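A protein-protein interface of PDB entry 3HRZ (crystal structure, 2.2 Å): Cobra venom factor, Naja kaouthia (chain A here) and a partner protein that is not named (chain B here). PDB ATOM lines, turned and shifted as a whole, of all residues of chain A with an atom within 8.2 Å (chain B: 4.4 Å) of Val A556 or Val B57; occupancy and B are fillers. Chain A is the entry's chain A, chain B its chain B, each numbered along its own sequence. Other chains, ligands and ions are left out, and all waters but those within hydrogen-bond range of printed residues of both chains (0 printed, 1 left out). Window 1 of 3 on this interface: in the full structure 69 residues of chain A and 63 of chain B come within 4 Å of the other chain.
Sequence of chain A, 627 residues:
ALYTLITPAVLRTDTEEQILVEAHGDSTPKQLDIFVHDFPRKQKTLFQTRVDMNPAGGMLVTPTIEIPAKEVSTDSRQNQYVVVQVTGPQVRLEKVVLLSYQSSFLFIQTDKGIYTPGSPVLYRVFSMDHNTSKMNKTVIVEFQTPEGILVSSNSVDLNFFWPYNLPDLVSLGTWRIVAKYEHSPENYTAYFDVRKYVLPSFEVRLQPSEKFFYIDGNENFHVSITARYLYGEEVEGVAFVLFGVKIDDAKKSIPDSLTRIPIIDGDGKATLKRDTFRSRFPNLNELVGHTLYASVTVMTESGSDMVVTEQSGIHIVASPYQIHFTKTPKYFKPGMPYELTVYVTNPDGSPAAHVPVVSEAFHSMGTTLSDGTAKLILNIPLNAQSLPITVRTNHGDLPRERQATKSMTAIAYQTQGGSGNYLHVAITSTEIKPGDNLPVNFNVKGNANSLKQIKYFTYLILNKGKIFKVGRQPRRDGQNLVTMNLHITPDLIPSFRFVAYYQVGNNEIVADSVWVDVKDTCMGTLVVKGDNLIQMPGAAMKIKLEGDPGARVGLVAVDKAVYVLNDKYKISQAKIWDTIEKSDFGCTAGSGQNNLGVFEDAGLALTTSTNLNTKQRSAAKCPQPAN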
ATOM      1  N   GLN A 109      -8.178 -11.733 -28.290  1.00  0.00           N
ATOM      2  CA  GLN A 109      -9.469 -11.086 -28.446  1.00  0.00           C
ATOM      3  C   GLN A 109      -9.238  -9.583 -28.606  1.00  0.00           C
ATOM      4  O   GLN A 109      -8.532  -8.986 -27.797  1.00  0.00           O
ATOM      5  CB  GLN A 109     -10.341 -11.305 -27.212  1.00  0.00           C
ATOM      6  CG  GLN A 109     -11.696 -10.572 -27.287  1.00  0.00           C
ATOM      7  CD  GLN A 109     -12.409 -10.536 -25.956  1.00  0.00           C
ATOM      8  OE1 GLN A 109     -11.780 -10.629 -24.897  1.00  0.00           O
ATOM      9  NE2 GLN A 109     -13.725 -10.393 -25.992  1.00  0.00           N
ATOM     10  N   THR A 110      -9.823  -8.982 -29.640  1.00  0.00           N
ATOM     11  CA  THR A 110      -9.879  -7.523 -29.748  1.00  0.00           C
ATOM     12  C   THR A 110     -11.311  -7.058 -29.465  1.00  0.00           C
ATOM     13  O   THR A 110     -12.258  -7.849 -29.574  1.00  0.00           O
ATOM     14  CB  THR A 110      -9.446  -7.007 -31.135  1.00  0.00           C
ATOM     15  OG1 THR A 110     -10.370  -7.464 -32.131  1.00  0.00           O
ATOM     16  CG2 THR A 110      -8.043  -7.475 -31.480  1.00  0.00           C
ATOM     17  N   ASP A 111     -11.474  -5.790 -29.089  1.00  0.00           N
ATOM     18  CA  ASP A 111     -12.808  -5.279 -28.775  1.00  0.00           C
ATOM     19  C   ASP A 111     -13.756  -5.271 -29.998  1.00  0.00           C
ATOM     20  O   ASP A 111     -14.955  -5.493 -29.848  1.00  0.00           O
ATOM     21  CB  ASP A 111     -12.751  -3.910 -28.051  1.00  0.00           C
ATOM     22  CG  ASP A 111     -12.199  -2.785 -28.927  1.00  0.00           C
ATOM     23  OD1 ASP A 111     -11.021  -2.844 -29.327  1.00  0.00           O
ATOM     24  OD2 ASP A 111     -12.944  -1.821 -29.192  1.00  0.00           O
ATOM     25  N   LYS A 112     -13.211  -5.058 -31.200  1.00  0.00           N
ATOM     26  CA  LYS A 112     -13.999  -5.069 -32.446  1.00  0.00           C
ATOM     27  C   LYS A 112     -13.196  -5.684 -33.586  1.00  0.00           C
ATOM     28  O   LYS A 112     -11.985  -5.832 -33.484  1.00  0.00           O
ATOM     29  CB  LYS A 112     -14.371  -3.632 -32.882  1.00  0.00           C
ATOM     30  CG  LYS A 112     -14.841  -2.714 -31.788  1.00  0.00           C
ATOM     31  CD  LYS A 112     -15.486  -1.457 -32.360  1.00  0.00           C
ATOM     32  CE  LYS A 112     -14.458  -0.399 -32.756  1.00  0.00           C
ATOM     33  NZ  LYS A 112     -13.718   0.066 -31.566  1.00  0.00           N
ATOM     34  N   LEU A 122      -8.225  -2.264 -28.434  1.00  0.00           N
ATOM     35  CA  LEU A 122      -8.104  -2.920 -27.145  1.00  0.00           C
ATOM     36  C   LEU A 122      -8.016  -4.433 -27.377  1.00  0.00           C
ATOM     37  O   LEU A 122      -8.742  -4.981 -28.200  1.00  0.00           O
ATOM     38  CB  LEU A 122      -9.295  -2.575 -26.252  1.00  0.00           C
ATOM     39  CG  LEU A 122      -9.549  -1.076 -26.023  1.00  0.00           C
ATOM     40  CD1 LEU A 122     -10.959  -0.835 -25.526  1.00  0.00           C
ATOM     41  CD2 LEU A 122      -8.559  -0.514 -25.065  1.00  0.00           C
ATOM     42  N   ARG A 124      -6.972  -8.564 -25.582  1.00  0.00           N
ATOM     43  CA  ARG A 124      -6.550  -9.482 -24.540  1.00  0.00           C
ATOM     44  C   ARG A 124      -5.909 -10.677 -25.210  1.00  0.00           C
ATOM     45  O   ARG A 124      -6.306 -11.063 -26.309  1.00  0.00           O
ATOM     46  CB  ARG A 124      -7.754  -9.997 -23.766  1.00  0.00           C
ATOM     47  CG  ARG A 124      -8.345  -9.013 -22.829  1.00  0.00           C
ATOM     48  CD  ARG A 124      -9.776  -9.385 -22.530  1.00  0.00           C
ATOM     49  NE  ARG A 124     -10.395  -8.350 -21.709  1.00  0.00           N
ATOM     50  CZ  ARG A 124     -11.676  -8.024 -21.761  1.00  0.00           C
ATOM     51  NH1 ARG A 124     -12.490  -8.652 -22.600  1.00  0.00           N
ATOM     52  NH2 ARG A 124     -12.132  -7.067 -20.971  1.00  0.00           N
ATOM     53  N   VAL A 528     -23.919 -15.659 -19.482  1.00  0.00           N
ATOM     54  CA  VAL A 528     -24.363 -14.313 -19.121  1.00  0.00           C
ATOM     55  C   VAL A 528     -25.891 -14.280 -19.132  1.00  0.00           C
ATOM     56  O   VAL A 528     -26.504 -14.431 -20.190  1.00  0.00           O
ATOM     57  CB  VAL A 528     -23.829 -13.263 -20.116  1.00  0.00           C
ATOM     58  CG1 VAL A 528     -24.352 -11.868 -19.771  1.00  0.00           C
ATOM     59  CG2 VAL A 528     -22.311 -13.286 -20.139  1.00  0.00           C
ATOM     60  N   LYS A 529     -26.501 -14.111 -17.960  1.00  0.00           N
ATOM     61  CA  LYS A 529     -27.959 -14.093 -17.839  1.00  0.00           C
ATOM     62  C   LYS A 529     -28.484 -12.698 -17.503  1.00  0.00           C
ATOM     63  O   LYS A 529     -27.910 -11.998 -16.675  1.00  0.00           O
ATOM     64  CB  LYS A 529     -28.424 -15.091 -16.778  1.00  0.00           C
ATOM     65  CG  LYS A 529     -28.253 -16.542 -17.177  1.00  0.00           C
ATOM     66  CD  LYS A 529     -28.223 -17.439 -15.959  1.00  0.00           C
ATOM     67  CE  LYS A 529     -28.179 -18.923 -16.340  1.00  0.00           C
ATOM     68  NZ  LYS A 529     -29.529 -19.554 -16.462  1.00  0.00           N
ATOM     69  N   MET A 541     -28.780  -1.493 -15.731  1.00  0.00           N
ATOM     70  CA  MET A 541     -28.805  -2.925 -16.022  1.00  0.00           C
ATOM     71  C   MET A 541     -28.263  -3.757 -14.870  1.00  0.00           C
ATOM     72  O   MET A 541     -27.456  -3.285 -14.066  1.00  0.00           O
ATOM     73  CB  MET A 541     -27.953  -3.237 -17.257  1.00  0.00           C
ATOM     74  CG  MET A 541     -28.433  -2.596 -18.530  1.00  0.00           C
ATOM     75  SD  MET A 541     -30.075  -3.150 -18.990  1.00  0.00           S
ATOM     76  CE  MET A 541     -29.827  -4.927 -19.088  1.00  0.00           C
ATOM     77  N   ILE A 543     -26.794  -7.869 -14.792  1.00  0.00           N
ATOM     78  CA  ILE A 543     -26.635  -9.179 -15.397  1.00  0.00           C
ATOM     79  C   ILE A 543     -25.909 -10.075 -14.404  1.00  0.00           C
ATOM     80  O   ILE A 543     -25.197  -9.594 -13.515  1.00  0.00           O
ATOM     81  CB  ILE A 543     -25.846  -9.120 -16.717  1.00  0.00           C
ATOM     82  CG1 ILE A 543     -24.446  -8.575 -16.466  1.00  0.00           C
ATOM     83  CG2 ILE A 543     -26.588  -8.287 -17.787  1.00  0.00           C
ATOM     84  CD1 ILE A 543     -23.645  -8.429 -17.729  1.00  0.00           C
ATOM     85  N   LEU A 545     -23.153 -13.127 -14.123  1.00  0.00           N
ATOM     86  CA  LEU A 545     -22.142 -13.959 -14.754  1.00  0.00           C
ATOM     87  C   LEU A 545     -22.072 -15.270 -13.977  1.00  0.00           C
ATOM     88  O   LEU A 545     -21.767 -15.272 -12.783  1.00  0.00           O
ATOM     89  CB  LEU A 545     -20.774 -13.275 -14.727  1.00  0.00           C
ATOM     90  CG  LEU A 545     -20.721 -11.791 -15.096  1.00  0.00           C
ATOM     91  CD1 LEU A 545     -19.319 -11.253 -14.856  1.00  0.00           C
ATOM     92  CD2 LEU A 545     -21.148 -11.572 -16.546  1.00  0.00           C
ATOM     93  N   VAL A 553     -13.032 -13.307 -15.851  1.00  0.00           N
ATOM     94  CA  VAL A 553     -13.911 -13.084 -16.985  1.00  0.00           C
ATOM     95  C   VAL A 553     -13.637 -11.739 -17.640  1.00  0.00           C
ATOM     96  O   VAL A 553     -13.845 -10.686 -17.023  1.00  0.00           O
ATOM     97  CB  VAL A 553     -15.372 -13.088 -16.542  1.00  0.00           C
ATOM     98  CG1 VAL A 553     -16.292 -13.010 -17.756  1.00  0.00           C
ATOM     99  CG2 VAL A 553     -15.665 -14.294 -15.688  1.00  0.00           C
ATOM    100  N   GLY A 554     -13.166 -11.766 -18.882  1.00  0.00           N
ATOM    101  CA  GLY A 554     -13.039 -10.541 -19.657  1.00  0.00           C
ATOM    102  C   GLY A 554     -14.360 -10.225 -20.331  1.00  0.00           C
ATOM    103  O   GLY A 554     -14.983 -11.105 -20.953  1.00  0.00           O
ATOM    104  N   LEU A 555     -14.807  -8.984 -20.199  1.00  0.00           N
ATOM    105  CA  LEU A 555     -16.074  -8.560 -20.795  1.00  0.00           C
ATOM    106  C   LEU A 555     -15.899  -7.507 -21.871  1.00  0.00           C
ATOM    107  O   LEU A 555     -14.843  -6.884 -21.971  1.00  0.00           O
ATOM    108  CB  LEU A 555     -16.975  -7.960 -19.735  1.00  0.00           C
ATOM    109  CG  LEU A 555     -17.416  -8.886 -18.616  1.00  0.00           C
ATOM    110  CD1 LEU A 555     -17.963  -8.034 -17.491  1.00  0.00           C
ATOM    111  CD2 LEU A 555     -18.483  -9.798 -19.145  1.00  0.00           C
ATOM    112  N   VAL A 556     -16.960  -7.310 -22.658  1.00  0.00           N
ATOM    113  CA  VAL A 556     -17.060  -6.213 -23.615  1.00  0.00           C
ATOM    114  C   VAL A 556     -18.505  -6.050 -24.091  1.00  0.00           C
ATOM    115  O   VAL A 556     -19.239  -7.034 -24.214  1.00  0.00           O
ATOM    116  CB  VAL A 556     -16.120  -6.410 -24.838  1.00  0.00           C
ATOM    117  CG1 VAL A 556     -16.636  -7.506 -25.765  1.00  0.00           C
ATOM    118  CG2 VAL A 556     -15.978  -5.110 -25.606  1.00  0.00           C
ATOM    119  N   ALA A 557     -18.923  -4.814 -24.356  1.00  0.00           N
ATOM    120  CA  ALA A 557     -20.236  -4.590 -24.956  1.00  0.00           C
ATOM    121  C   ALA A 557     -20.025  -3.961 -26.323  1.00  0.00           C
ATOM    122  O   ALA A 557     -19.350  -2.929 -26.437  1.00  0.00           O
ATOM    123  CB  ALA A 557     -21.101  -3.700 -24.068  1.00  0.00           C
ATOM    124  N   VAL A 558     -20.585  -4.578 -27.361  1.00  0.00           N
ATOM    125  CA  VAL A 558     -20.373  -4.094 -28.726  1.00  0.00           C
ATOM    126  C   VAL A 558     -21.692  -3.723 -29.392  1.00  0.00           C
ATOM    127  O   VAL A 558     -22.676  -4.458 -29.257  1.00  0.00           O
ATOM    128  CB  VAL A 558     -19.671  -5.156 -29.585  1.00  0.00           C
ATOM    129  CG1 VAL A 558     -19.210  -4.554 -30.917  1.00  0.00           C
ATOM    130  CG2 VAL A 558     -18.491  -5.728 -28.835  1.00  0.00           C
ATOM    131  N   ASP A 559     -21.723  -2.579 -30.085  1.00  0.00           N
ATOM    132  CA  ASP A 559     -22.893  -2.220 -30.898  1.00  0.00           C
ATOM    133  C   ASP A 559     -23.049  -3.294 -31.977  1.00  0.00           C
ATOM    134  O   ASP A 559     -22.111  -3.572 -32.743  1.00  0.00           O
ATOM    135  CB  ASP A 559     -22.729  -0.849 -31.570  1.00  0.00           C
ATOM    136  CG  ASP A 559     -24.065  -0.241 -32.040  1.00  0.00           C
ATOM    137  OD1 ASP A 559     -24.934  -0.963 -32.583  1.00  0.00           O
ATOM    138  OD2 ASP A 559     -24.239   0.992 -31.871  1.00  0.00           O
ATOM    139  N   LYS A 560     -24.228  -3.887 -32.036  1.00  0.00           N
ATOM    140  CA  LYS A 560     -24.478  -4.925 -33.014  1.00  0.00           C
ATOM    141  C   LYS A 560     -24.209  -4.364 -34.422  1.00  0.00           C
ATOM    142  O   LYS A 560     -23.886  -5.105 -35.344  1.00  0.00           O
ATOM    143  CB  LYS A 560     -25.910  -5.426 -32.874  1.00  0.00           C
ATOM    144  CG  LYS A 560     -26.187  -6.798 -33.467  1.00  0.00           C
ATOM    145  CD  LYS A 560     -27.694  -7.074 -33.479  1.00  0.00           C
ATOM    146  CE  LYS A 560     -28.029  -8.437 -34.067  1.00  0.00           C
ATOM    147  NZ  LYS A 560     -27.182  -9.483 -33.429  1.00  0.00           N
ATOM    148  N   TYR A 563     -20.932  -5.434 -36.213  1.00  0.00           N
ATOM    149  CA  TYR A 563     -20.906  -6.729 -36.909  1.00  0.00           C
ATOM    150  C   TYR A 563     -21.428  -6.674 -38.327  1.00  0.00           C
ATOM    151  O   TYR A 563     -21.038  -7.498 -39.159  1.00  0.00           O
ATOM    152  CB  TYR A 563     -21.657  -7.802 -36.122  1.00  0.00           C
ATOM    153  CG  TYR A 563     -21.030  -8.041 -34.779  1.00  0.00           C
ATOM    154  CD1 TYR A 563     -19.660  -7.930 -34.617  1.00  0.00           C
ATOM    155  CD2 TYR A 563     -21.800  -8.361 -33.671  1.00  0.00           C
ATOM    156  CE1 TYR A 563     -19.061  -8.141 -33.385  1.00  0.00           C
ATOM    157  CE2 TYR A 563     -21.219  -8.578 -32.435  1.00  0.00           C
ATOM    158  CZ  TYR A 563     -19.845  -8.467 -32.297  1.00  0.00           C
ATOM    159  OH  TYR A 563     -19.247  -8.680 -31.075  1.00  0.00           O
ATOM    160  N   LYS A 570     -13.937 -12.465 -35.192  1.00  0.00           N
ATOM    161  CA  LYS A 570     -14.299 -12.608 -33.786  1.00  0.00           C
ATOM    162  C   LYS A 570     -13.749 -13.906 -33.174  1.00  0.00           C
ATOM    163  O   LYS A 570     -13.745 -14.943 -33.830  1.00  0.00           O
ATOM    164  CB  LYS A 570     -15.829 -12.565 -33.658  1.00  0.00           C
ATOM    165  CG  LYS A 570     -16.372 -12.879 -32.270  1.00  0.00           C
ATOM    166  CD  LYS A 570     -17.901 -12.837 -32.245  1.00  0.00           C
ATOM    167  CE  LYS A 570     -18.471 -13.179 -30.860  1.00  0.00           C
ATOM    168  NZ  LYS A 570     -18.307 -14.617 -30.463  1.00  0.00           N
ATOM    169  N   ILE A 571     -13.284 -13.848 -31.926  1.00  0.00           N
ATOM    170  CA  ILE A 571     -12.961 -15.074 -31.191  1.00  0.00           C
ATOM    171  C   ILE A 571     -14.235 -15.887 -30.897  1.00  0.00           C
ATOM    172  O   ILE A 571     -15.307 -15.324 -30.712  1.00  0.00           O
ATOM    173  CB  ILE A 571     -12.218 -14.770 -29.873  1.00  0.00           C
ATOM    174  CG1 ILE A 571     -11.562 -16.036 -29.315  1.00  0.00           C
ATOM    175  CG2 ILE A 571     -13.167 -14.171 -28.835  1.00  0.00           C
ATOM    176  CD1 ILE A 571     -10.695 -15.771 -28.085  1.00  0.00           C
ATOM    177  N   TRP B  23     -17.667  -0.777 -25.553  1.00  0.00           N
ATOM    178  CA  TRP B  23     -17.498  -0.252 -24.209  1.00  0.00           C
ATOM    179  C   TRP B  23     -17.513  -1.413 -23.217  1.00  0.00           C
ATOM    180  O   TRP B  23     -17.479  -2.582 -23.629  1.00  0.00           O
ATOM    181  CB  TRP B  23     -18.575   0.796 -23.896  1.00  0.00           C
ATOM    182  CG  TRP B  23     -19.981   0.328 -24.077  1.00  0.00           C
ATOM    183  CD1 TRP B  23     -20.614   0.057 -25.259  1.00  0.00           C
ATOM    184  CD2 TRP B  23     -20.946   0.094 -23.042  1.00  0.00           C
ATOM    185  NE1 TRP B  23     -21.912  -0.336 -25.022  1.00  0.00           N
ATOM    186  CE2 TRP B  23     -22.136  -0.335 -23.668  1.00  0.00           C
ATOM    187  CE3 TRP B  23     -20.913   0.188 -21.649  1.00  0.00           C
ATOM    188  CZ2 TRP B  23     -23.285  -0.664 -22.947  1.00  0.00           C
ATOM    189  CZ3 TRP B  23     -22.052  -0.129 -20.935  1.00  0.00           C
ATOM    190  CH2 TRP B  23     -23.223  -0.552 -21.585  1.00  0.00           C
ATOM    191  N   LEU B  24     -17.526  -1.107 -21.922  1.00  0.00           N
ATOM    192  CA  LEU B  24     -17.554  -2.155 -20.894  1.00  0.00           C
ATOM    193  C   LEU B  24     -16.387  -3.145 -21.009  1.00  0.00           C
ATOM    194  O   LEU B  24     -16.575  -4.351 -20.858  1.00  0.00           O
ATOM    195  CB  LEU B  24     -18.863  -2.942 -20.985  1.00  0.00           C
ATOM    196  CG  LEU B  24     -19.347  -3.558 -19.673  1.00  0.00           C
ATOM    197  CD1 LEU B  24     -19.717  -2.456 -18.693  1.00  0.00           C
ATOM    198  CD2 LEU B  24     -20.527  -4.451 -19.929  1.00  0.00           C
ATOM    199  N   TRP B  25     -15.196  -2.634 -21.292  1.00  0.00           N
ATOM    200  CA  TRP B  25     -14.008  -3.465 -21.439  1.00  0.00           C
ATOM    201  C   TRP B  25     -13.384  -3.672 -20.051  1.00  0.00           C
ATOM    202  O   TRP B  25     -12.409  -3.018 -19.682  1.00  0.00           O
ATOM    203  CB  TRP B  25     -13.033  -2.782 -22.397  1.00  0.00           C
ATOM    204  CG  TRP B  25     -11.776  -3.562 -22.749  1.00  0.00           C
ATOM    205  CD1 TRP B  25     -10.516  -3.354 -22.250  1.00  0.00           C
ATOM    206  CD2 TRP B  25     -11.659  -4.642 -23.694  1.00  0.00           C
ATOM    207  NE1 TRP B  25      -9.627  -4.236 -22.822  1.00  0.00           N
ATOM    208  CE2 TRP B  25     -10.300  -5.035 -23.713  1.00  0.00           C
ATOM    209  CE3 TRP B  25     -12.562  -5.286 -24.553  1.00  0.00           C
ATOM    210  CZ2 TRP B  25      -9.826  -6.063 -24.538  1.00  0.00           C
ATOM    211  CZ3 TRP B  25     -12.089  -6.321 -25.379  1.00  0.00           C
ATOM    212  CH2 TRP B  25     -10.735  -6.694 -25.362  1.00  0.00           C
ATOM    213  N   TRP B  55     -27.191  -4.016 -28.138  1.00  0.00           N
ATOM    214  CA  TRP B  55     -25.828  -4.265 -27.707  1.00  0.00           C
ATOM    215  C   TRP B  55     -25.639  -5.772 -27.591  1.00  0.00           C
ATOM    216  O   TRP B  55     -26.578  -6.510 -27.308  1.00  0.00           O
ATOM    217  CB  TRP B  55     -25.536  -3.633 -26.352  1.00  0.00           C
ATOM    218  CG  TRP B  55     -25.743  -2.173 -26.272  1.00  0.00           C
ATOM    219  CD1 TRP B  55     -26.770  -1.534 -25.642  1.00  0.00           C
ATOM    220  CD2 TRP B  55     -24.897  -1.140 -26.817  1.00  0.00           C
ATOM    221  NE1 TRP B  55     -26.625  -0.177 -25.769  1.00  0.00           N
ATOM    222  CE2 TRP B  55     -25.487   0.094 -26.486  1.00  0.00           C
ATOM    223  CE3 TRP B  55     -23.709  -1.144 -27.563  1.00  0.00           C
ATOM    224  CZ2 TRP B  55     -24.921   1.329 -26.862  1.00  0.00           C
ATOM    225  CZ3 TRP B  55     -23.144   0.079 -27.930  1.00  0.00           C
ATOM    226  CH2 TRP B  55     -23.756   1.297 -27.580  1.00  0.00           C
ATOM    227  N   VAL B  56     -24.410  -6.212 -27.797  1.00  0.00           N
ATOM    228  CA  VAL B  56     -24.040  -7.591 -27.581  1.00  0.00           C
ATOM    229  C   VAL B  56     -22.960  -7.603 -26.504  1.00  0.00           C
ATOM    230  O   VAL B  56     -21.870  -7.066 -26.700  1.00  0.00           O
ATOM    231  CB  VAL B  56     -23.511  -8.202 -28.882  1.00  0.00           C
ATOM    232  CG1 VAL B  56     -23.296  -9.673 -28.722  1.00  0.00           C
ATOM    233  CG2 VAL B  56     -24.506  -7.946 -30.015  1.00  0.00           C
ATOM    234  N   VAL B  57     -23.291  -8.167 -25.349  1.00  0.00           N
ATOM    235  CA  VAL B  57     -22.324  -8.359 -24.283  1.00  0.00           C
ATOM    236  C   VAL B  57     -21.614  -9.706 -24.436  1.00  0.00           C
ATOM    237  O   VAL B  57     -22.249 -10.760 -24.413  1.00  0.00           O
ATOM    238  CB  VAL B  57     -22.993  -8.316 -22.912  1.00  0.00           C
ATOM    239  CG1 VAL B  57     -21.966  -8.619 -21.827  1.00  0.00           C
ATOM    240  CG2 VAL B  57     -23.636  -6.947 -22.683  1.00  0.00           C
ATOM    241  N   LEU B  58     -20.295  -9.661 -24.588  1.00  0.00           N
ATOM    242  CA  LEU B  58     -19.489 -10.859 -24.762  1.00  0.00           C
ATOM    243  C   LEU B  58     -18.586 -11.108 -23.542  1.00  0.00           C
ATOM    244  O   LEU B  58     -17.843 -10.222 -23.095  1.00  0.00           O
ATOM    245  CB  LEU B  58     -18.631 -10.715 -26.012  1.00  0.00           C
ATOM    246  CG  LEU B  58     -19.417 -10.276 -27.248  1.00  0.00           C
ATOM    247  CD1 LEU B  58     -18.528  -9.555 -28.243  1.00  0.00           C
ATOM    248  CD2 LEU B  58     -20.099 -11.469 -27.894  1.00  0.00           C
ATOM    249  N   ALA B  59     -18.651 -12.318 -23.010  1.00  0.00           N
ATOM    250  CA  ALA B  59     -17.780 -12.710 -21.913  1.00  0.00           C
ATOM    251  C   ALA B  59     -16.859 -13.852 -22.326  1.00  0.00           C
ATOM    252  O   ALA B  59     -17.276 -14.786 -23.002  1.00  0.00           O
ATOM    253  CB  ALA B  59     -18.604 -13.095 -20.694  1.00  0.00           C
ATOM    254  N   PRO B  73     -23.269 -14.893 -26.891  1.00  0.00           N
ATOM    255  CA  PRO B  73     -23.570 -13.460 -26.771  1.00  0.00           C
ATOM    256  C   PRO B  73     -24.884 -13.222 -26.041  1.00  0.00           C
ATOM    257  O   PRO B  73     -25.844 -13.979 -26.214  1.00  0.00           O
ATOM    258  CB  PRO B  73     -23.695 -12.998 -28.224  1.00  0.00           C
ATOM    259  CG  PRO B  73     -22.948 -14.028 -29.016  1.00  0.00           C
ATOM    260  CD  PRO B  73     -23.185 -15.323 -28.298  1.00  0.00           C
ATOM    261  N   TYR B  74     -24.909 -12.195 -25.202  1.00  0.00           N
ATOM    262  CA  TYR B  74     -26.153 -11.758 -24.579  1.00  0.00           C
ATOM    263  C   TYR B  74     -26.568 -10.414 -25.185  1.00  0.00           C
ATOM    264  O   TYR B  74     -25.813  -9.442 -25.159  1.00  0.00           O
ATOM    265  CB  TYR B  74     -26.017 -11.660 -23.055  1.00  0.00           C
ATOM    266  CG  TYR B  74     -27.238 -11.066 -22.392  1.00  0.00           C
ATOM    267  CD1 TYR B  74     -28.385 -11.823 -22.197  1.00  0.00           C
ATOM    268  CD2 TYR B  74     -27.242  -9.747 -21.967  1.00  0.00           C
ATOM    269  CE1 TYR B  74     -29.508 -11.272 -21.600  1.00  0.00           C
ATOM    270  CE2 TYR B  74     -28.354  -9.190 -21.374  1.00  0.00           C
ATOM    271  CZ  TYR B  74     -29.485  -9.952 -21.194  1.00  0.00           C
ATOM    272  OH  TYR B  74     -30.593  -9.386 -20.598  1.00  0.00           O
ATOM    273  N   ILE B  76     -28.790  -6.989 -25.609  1.00  0.00           N
ATOM    274  CA  ILE B  76     -29.604  -6.030 -24.908  1.00  0.00           C
ATOM    275  C   ILE B  76     -30.251  -5.177 -25.986  1.00  0.00           C
ATOM    276  O   ILE B  76     -29.571  -4.550 -26.788  1.00  0.00           O
ATOM    277  CB  ILE B  76     -28.737  -5.119 -24.013  1.00  0.00           C
ATOM    278  CG1 ILE B  76     -28.030  -5.926 -22.935  1.00  0.00           C
ATOM    279  CG2 ILE B  76     -29.578  -4.028 -23.380  1.00  0.00           C
ATOM    280  CD1 ILE B  76     -26.916  -5.136 -22.240  1.00  0.00           C
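Of the printed residues of chain B, Arg A124 touches Trp B25 (3.6 Å). Val A556 touches just these residues of chain B: Trp B23 (3.5 Å), Leu B24 (3.4 Å), Trp B25 (3.6 Å), Val B56 (3.6 Å), Val B57 (3.4 Å) and Leu B58 (2.9 Å). Printed residues of chain B within 4 Å of Lys A570: Leu B58 (3.8 Å). Printed residues of chain A within 4 Å of Trp B55: Val A558 (3.5 Å) and Asp A559 (3.5 Å). Printed residues of chain A within 4 Å of Val B57: Val A556 (3.4 Å). Of the printed residues of chain A, Leu B58 touches Gly A554 (3.7 Å), Leu A555 (3.3 Å), Val A556 (2.9 Å), Val A558 (3.9 Å), Tyr A563 (3.1 Å) and Lys A570 (3.8 Å). The nearest residue of chain A that does not touch Val B57 is Ala A557 (4.3 Å). The nearest printed residue of chain A that does not touch Leu B58 is Gln A109 (4.9 Å).
Among the printed residues, merely in contact across the chains: Asp A111 with Trp B25 (3.6 Å), Leu A122 with Trp B25 (3.7 Å), Arg A124 with Trp B25 (3.6 Å), Val A528 with Ala B59 (3.8 Å), Val A528 with Tyr B74 (3.7 Å), Val A553 with Ala B59 (3.7 Å), Gly A554 with Leu B58 (3.7 Å), Gly A554 with Ala B59 (3.4 Å), Leu A555 with Trp B25 (3.6 Å), Leu A555 with Leu B58 (3.3 Å), Leu A555 with Ala B59 (3.6 Å), Val A556 with Trp B23 (3.5 Å), Val A556 with Trp B25 (3.6 Å), Val A556 with Val B56 (3.6 Å), Val A556 with Val B57 (3.4 Å), Ala A557 with Leu B24 (3.9 Å), Ala A557 with Val B56 (3.4 Å), Val A558 with Trp B55 (3.5 Å), Val A558 with Leu B58 (3.9 Å), Asp A559 with Trp B55 (3.5 Å), Tyr A563 with Leu B58 (3.1 Å) and Lys A570 with Leu B58 (3.8 Å).
The backbone NH of Val B57 lies within hydrogen-bond range of the backbone carbonyl oxygen of Tyr B74 (2.8 Å). N of Asp A111 is in hydrogen-bond range of O of Leu A122 (3.0 Å). O of Gln A109 is in hydrogen-bond range of N of Arg A124 (2.7 Å). The side-chain carboxylate of Asp A111 is in salt-bridge range of the side-chain amino group of Lys A112. The backbone NH (N) of Trp B55 is in hydrogen-bond range of the backbone carbonyl oxygen (O) of Ile B76 (2.8 Å). The guanidinium group (NH2) of Arg A124 sits at hydrogen-bond distance from the backbone carbonyl oxygen (O) of Leu A555, at 2.9 Å.
Of the 11 printed residues of chain B, 9 touch a printed residue of chain A. Among the printed residues, 27 pairs touch across the chains.
The backbone carbonyl oxygen (O) of Val A558 is in hydrogen-bond range of the backbone NH (N) of Val B56 (2.9 Å). The backbone carbonyl oxygen (O) of Trp B23 is in hydrogen-bond range of the backbone NH (N) of Ala A557 (2.8 Å). The backbone carbonyl oxygen of Leu B24 lies close to the backbone carbonyl oxygen of Leu A555 (3.3 Å). N of Val A556 lies close to O of Leu B24 (3.5 Å). The backbone carbonyl oxygen of Val A556 sits at hydrogen-bond distance from the backbone NH of Leu B58 (2.9 Å).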
